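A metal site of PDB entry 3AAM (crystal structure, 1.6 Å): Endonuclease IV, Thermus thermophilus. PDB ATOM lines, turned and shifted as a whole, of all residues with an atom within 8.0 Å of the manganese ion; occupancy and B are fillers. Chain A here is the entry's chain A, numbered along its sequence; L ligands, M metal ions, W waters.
The backbone NH (N) of His 172 lies within hydrogen-bond range of the side-chain carboxylate (OD1) of Asp 169 (2.9 Å). O of Asn 140 is in hydrogen-bond range of ND1 of His 172, 2.7 Å away. A ring nitrogen (ND1) of His 219 sits at hydrogen-bond distance from the backbone carbonyl oxygen of Glu 248, 2.8 Å away. OD1 of Asn 206 sits close to ND1 of His 219, at 3.4 Å.
Three residues have an atom within 4 Å of the manganese ion: His 172, Asp 217 and His 219.
O3 of the ligand binds the manganese ion (2.0 Å). The manganese ion is bound by NE2 of His 172 (2.2 Å). The manganese ion is bound by NE2 of His 219. OD1 of Asp 217 is bound to the manganese ion (2.4 Å). The manganese ion is bound by the side-chain carboxylate (OD2) of Asp 217 (2.5 Å). The manganese ion is bound by water W1. The manganese ion has six donor atoms within binding distance.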
ATOM      1  N   HIS A  69      29.010 -17.107 -17.330  1.00  0.00           N
ATOM      2  CA  HIS A  69      28.433 -15.819 -17.671  1.00  0.00           C
ATOM      3  C   HIS A  69      27.633 -15.952 -18.968  1.00  0.00           C
ATOM      4  O   HIS A  69      28.100 -16.556 -19.927  1.00  0.00           O
ATOM      5  CB  HIS A  69      29.539 -14.773 -17.880  1.00  0.00           C
ATOM      6  CG  HIS A  69      29.085 -13.359 -17.728  1.00  0.00           C
ATOM      7  ND1 HIS A  69      28.052 -12.818 -18.471  1.00  0.00           N
ATOM      8  CD2 HIS A  69      29.508 -12.364 -16.906  1.00  0.00           C
ATOM      9  CE1 HIS A  69      27.861 -11.566 -18.104  1.00  0.00           C
ATOM     10  NE2 HIS A  69      28.735 -11.265 -17.165  1.00  0.00           N
ATOM     11  N   HIS A 108      23.085 -10.225 -17.229  1.00  0.00           N
ATOM     12  CA  HIS A 108      22.683  -8.853 -16.969  1.00  0.00           C
ATOM     13  C   HIS A 108      21.173  -8.848 -17.209  1.00  0.00           C
ATOM     14  O   HIS A 108      20.663  -9.624 -18.021  1.00  0.00           O
ATOM     15  CB  HIS A 108      23.451  -7.857 -17.861  1.00  0.00           C
ATOM     16  CG  HIS A 108      23.295  -8.074 -19.338  1.00  0.00           C
ATOM     17  ND1 HIS A 108      23.942  -7.276 -20.266  1.00  0.00           N
ATOM     18  CD2 HIS A 108      22.576  -8.972 -20.046  1.00  0.00           C
ATOM     19  CE1 HIS A 108      23.628  -7.686 -21.482  1.00  0.00           C
ATOM     20  NE2 HIS A 108      22.794  -8.710 -21.376  1.00  0.00           N
ATOM     21  N   GLU A 139      22.648  -9.397 -12.327  1.00  0.00           N
ATOM     22  CA  GLU A 139      23.571  -8.327 -11.954  1.00  0.00           C
ATOM     23  C   GLU A 139      22.888  -6.982 -11.881  1.00  0.00           C
ATOM     24  O   GLU A 139      21.901  -6.732 -12.570  1.00  0.00           O
ATOM     25  CB  GLU A 139      24.701  -8.198 -12.995  1.00  0.00           C
ATOM     26  CG  GLU A 139      25.116  -9.488 -13.681  1.00  0.00           C
ATOM     27  CD  GLU A 139      26.127  -9.258 -14.805  1.00  0.00           C
ATOM     28  OE1 GLU A 139      25.998  -8.265 -15.550  1.00  0.00           O
ATOM     29  OE2 GLU A 139      27.040 -10.098 -14.965  1.00  0.00           O
ATOM     30  N   ASN A 140      23.419  -6.102 -11.041  1.00  0.00           N
ATOM     31  CA  ASN A 140      22.894  -4.749 -10.975  1.00  0.00           C
ATOM     32  C   ASN A 140      23.561  -4.090 -12.186  1.00  0.00           C
ATOM     33  O   ASN A 140      24.592  -4.575 -12.669  1.00  0.00           O
ATOM     34  CB  ASN A 140      23.321  -4.040  -9.689  1.00  0.00           C
ATOM     35  CG  ASN A 140      24.818  -4.036  -9.494  1.00  0.00           C
ATOM     36  OD1 ASN A 140      25.429  -5.086  -9.317  1.00  0.00           O
ATOM     37  ND2 ASN A 140      25.422  -2.846  -9.510  1.00  0.00           N
ATOM     38  N   THR A 141      22.977  -3.016 -12.691  1.00  0.00           N
ATOM     39  CA  THR A 141      23.518  -2.347 -13.876  1.00  0.00           C
ATOM     40  C   THR A 141      23.820  -0.867 -13.691  1.00  0.00           C
ATOM     41  O   THR A 141      23.494  -0.281 -12.667  1.00  0.00           O
ATOM     42  CB  THR A 141      22.542  -2.484 -15.058  1.00  0.00           C
ATOM     43  OG1 THR A 141      21.340  -1.763 -14.762  1.00  0.00           O
ATOM     44  CG2 THR A 141      22.192  -3.951 -15.285  1.00  0.00           C
ATOM     45  N   ALA A 142      24.439  -0.286 -14.713  1.00  0.00           N
ATOM     46  CA  ALA A 142      24.788   1.123 -14.707  1.00  0.00           C
ATOM     47  C   ALA A 142      23.528   1.979 -14.848  1.00  0.00           C
ATOM     48  O   ALA A 142      23.536   3.170 -14.552  1.00  0.00           O
ATOM     49  CB  ALA A 142      25.762   1.428 -15.837  1.00  0.00           C
ATOM     50  N   ASP A 169      28.020  -5.932  -9.168  1.00  0.00           N
ATOM     51  CA  ASP A 169      29.123  -5.464 -10.006  1.00  0.00           C
ATOM     52  C   ASP A 169      29.410  -4.053  -9.494  1.00  0.00           C
ATOM     53  O   ASP A 169      28.567  -3.158  -9.578  1.00  0.00           O
ATOM     54  CB  ASP A 169      28.738  -5.430 -11.482  1.00  0.00           C
ATOM     55  CG  ASP A 169      29.907  -5.021 -12.369  1.00  0.00           C
ATOM     56  OD1 ASP A 169      30.486  -3.942 -12.130  1.00  0.00           O
ATOM     57  OD2 ASP A 169      30.256  -5.782 -13.305  1.00  0.00           O
ATOM     58  N   CYS A 171      31.504  -1.812 -10.662  1.00  0.00           N
ATOM     59  CA  CYS A 171      31.634  -0.818 -11.718  1.00  0.00           C
ATOM     60  C   CYS A 171      30.235  -0.329 -12.059  1.00  0.00           C
ATOM     61  O   CYS A 171      29.986   0.881 -12.151  1.00  0.00           O
ATOM     62  CB  CYS A 171      32.278  -1.425 -12.968  1.00  0.00           C
ATOM     63  SG  CYS A 171      32.353  -0.303 -14.400  1.00  0.00           S
ATOM     64  N   HIS A 172      29.321  -1.265 -12.247  1.00  0.00           N
ATOM     65  CA  HIS A 172      27.935  -0.912 -12.568  1.00  0.00           C
ATOM     66  C   HIS A 172      27.328  -0.047 -11.471  1.00  0.00           C
ATOM     67  O   HIS A 172      26.663   0.946 -11.748  1.00  0.00           O
ATOM     68  CB  HIS A 172      27.084  -2.177 -12.724  1.00  0.00           C
ATOM     69  CG  HIS A 172      27.485  -3.030 -13.893  1.00  0.00           C
ATOM     70  ND1 HIS A 172      26.854  -4.218 -14.178  1.00  0.00           N
ATOM     71  CD2 HIS A 172      28.455  -2.874 -14.824  1.00  0.00           C
ATOM     72  CE1 HIS A 172      27.417  -4.764 -15.247  1.00  0.00           C
ATOM     73  NE2 HIS A 172      28.392  -3.965 -15.660  1.00  0.00           N
ATOM     74  N   HIS A 204      31.283  -9.098  -9.053  1.00  0.00           N
ATOM     75  CA  HIS A 204      32.118  -8.781 -10.213  1.00  0.00           C
ATOM     76  C   HIS A 204      32.822  -7.510  -9.722  1.00  0.00           C
ATOM     77  O   HIS A 204      32.263  -6.410  -9.787  1.00  0.00           O
ATOM     78  CB  HIS A 204      31.281  -8.502 -11.461  1.00  0.00           C
ATOM     79  CG  HIS A 204      30.759  -9.725 -12.148  1.00  0.00           C
ATOM     80  ND1 HIS A 204      31.384 -10.955 -12.043  1.00  0.00           N
ATOM     81  CD2 HIS A 204      29.703  -9.902 -12.963  1.00  0.00           C
ATOM     82  CE1 HIS A 204      30.719 -11.832 -12.778  1.00  0.00           C
ATOM     83  NE2 HIS A 204      29.703 -11.222 -13.350  1.00  0.00           N
ATOM     84  N   ASN A 206      34.819  -5.199 -10.591  1.00  0.00           N
ATOM     85  CA  ASN A 206      35.362  -4.380 -11.656  1.00  0.00           C
ATOM     86  C   ASN A 206      35.590  -2.933 -11.231  1.00  0.00           C
ATOM     87  O   ASN A 206      34.756  -2.359 -10.537  1.00  0.00           O
ATOM     88  CB  ASN A 206      34.393  -4.376 -12.847  1.00  0.00           C
ATOM     89  CG  ASN A 206      34.218  -5.738 -13.458  1.00  0.00           C
ATOM     90  OD1 ASN A 206      33.103  -6.191 -13.707  1.00  0.00           O
ATOM     91  ND2 ASN A 206      35.329  -6.412 -13.721  1.00  0.00           N
ATOM     92  N   ASP A 207      36.713  -2.354 -11.628  1.00  0.00           N
ATOM     93  CA  ASP A 207      36.908  -0.945 -11.316  1.00  0.00           C
ATOM     94  C   ASP A 207      36.193  -0.261 -12.474  1.00  0.00           C
ATOM     95  O   ASP A 207      35.760  -0.933 -13.413  1.00  0.00           O
ATOM     96  CB  ASP A 207      38.391  -0.547 -11.269  1.00  0.00           C
ATOM     97  CG  ASP A 207      38.611   0.751 -10.505  1.00  0.00           C
ATOM     98  OD1 ASP A 207      37.710   1.618 -10.517  1.00  0.00           O
ATOM     99  OD2 ASP A 207      39.695   0.910  -9.896  1.00  0.00           O
ATOM    100  N   VAL A 216      28.155   5.156 -17.381  1.00  0.00           N
ATOM    101  CA  VAL A 216      29.125   4.550 -18.295  1.00  0.00           C
ATOM    102  C   VAL A 216      29.541   3.191 -17.729  1.00  0.00           C
ATOM    103  O   VAL A 216      29.931   3.092 -16.552  1.00  0.00           O
ATOM    104  CB  VAL A 216      30.376   5.441 -18.459  1.00  0.00           C
ATOM    105  CG1 VAL A 216      31.451   4.693 -19.248  1.00  0.00           C
ATOM    106  CG2 VAL A 216      30.001   6.723 -19.182  1.00  0.00           C
ATOM    107  N   ASP A 217      29.451   2.153 -18.552  1.00  0.00           N
ATOM    108  CA  ASP A 217      29.819   0.801 -18.148  1.00  0.00           C
ATOM    109  C   ASP A 217      31.115   0.430 -18.876  1.00  0.00           C
ATOM    110  O   ASP A 217      31.079  -0.138 -19.965  1.00  0.00           O
ATOM    111  CB  ASP A 217      28.709  -0.181 -18.514  1.00  0.00           C
ATOM    112  CG  ASP A 217      29.030  -1.621 -18.120  1.00  0.00           C
ATOM    113  OD1 ASP A 217      30.049  -1.846 -17.449  1.00  0.00           O
ATOM    114  OD2 ASP A 217      28.251  -2.532 -18.487  1.00  0.00           O
ATOM    115  N   HIS A 218      32.239   0.761 -18.256  1.00  0.00           N
ATOM    116  CA  HIS A 218      33.551   0.496 -18.842  1.00  0.00           C
ATOM    117  C   HIS A 218      34.472  -0.015 -17.734  1.00  0.00           C
ATOM    118  O   HIS A 218      34.978   0.768 -16.926  1.00  0.00           O
ATOM    119  CB  HIS A 218      34.077   1.809 -19.451  1.00  0.00           C
ATOM    120  CG  HIS A 218      35.295   1.648 -20.305  1.00  0.00           C
ATOM    121  ND1 HIS A 218      35.825   2.683 -21.042  1.00  0.00           N
ATOM    122  CD2 HIS A 218      36.100   0.580 -20.526  1.00  0.00           C
ATOM    123  CE1 HIS A 218      36.898   2.264 -21.682  1.00  0.00           C
ATOM    124  NE2 HIS A 218      37.084   0.992 -21.399  1.00  0.00           N
ATOM    125  N   HIS A 219      34.676  -1.326 -17.685  1.00  0.00           N
ATOM    126  CA  HIS A 219      35.506  -1.932 -16.651  1.00  0.00           C
ATOM    127  C   HIS A 219      36.968  -1.511 -16.738  1.00  0.00           C
ATOM    128  O   HIS A 219      37.481  -1.223 -17.825  1.00  0.00           O
ATOM    129  CB  HIS A 219      35.469  -3.468 -16.746  1.00  0.00           C
ATOM    130  CG  HIS A 219      34.097  -4.051 -16.767  1.00  0.00           C
ATOM    131  ND1 HIS A 219      33.876  -5.399 -16.946  1.00  0.00           N
ATOM    132  CD2 HIS A 219      32.865  -3.483 -16.666  1.00  0.00           C
ATOM    133  CE1 HIS A 219      32.574  -5.635 -16.952  1.00  0.00           C
ATOM    134  NE2 HIS A 219      31.939  -4.496 -16.784  1.00  0.00           N
ATOM    135  N   GLU A 248      36.525  -8.802 -14.426  1.00  0.00           N
ATOM    136  CA  GLU A 248      36.221  -8.971 -15.847  1.00  0.00           C
ATOM    137  C   GLU A 248      36.897  -7.862 -16.652  1.00  0.00           C
ATOM    138  O   GLU A 248      36.268  -6.875 -17.012  1.00  0.00           O
ATOM    139  CB  GLU A 248      34.703  -8.908 -16.061  1.00  0.00           C
ATOM    140  CG  GLU A 248      33.895  -9.849 -15.187  1.00  0.00           C
ATOM    141  CD  GLU A 248      32.395  -9.688 -15.410  1.00  0.00           C
ATOM    142  OE1 GLU A 248      31.924  -8.535 -15.377  1.00  0.00           O
ATOM    143  OE2 GLU A 248      31.709 -10.704 -15.614  1.00  0.00           O
HETATM  144  P1  LIG L   1      28.973  -7.674 -17.625  1.00  0.00           P
HETATM  145  O1  LIG L   1      29.714  -8.044 -18.963  1.00  0.00           O
HETATM  146  O2  LIG L   1      29.538  -8.574 -16.447  1.00  0.00           O
HETATM  147  O3  LIG L   1      29.216  -6.172 -17.290  1.00  0.00           O
HETATM  148  O4  LIG L   1      27.427  -7.928 -17.794  1.00  0.00           O
HETATM  149 MN    MN M   1      29.759  -4.204 -17.422  1.00  0.00          MN
HETATM  150  O   HOH W   1      30.625  -4.342 -19.767  1.00  0.00           O
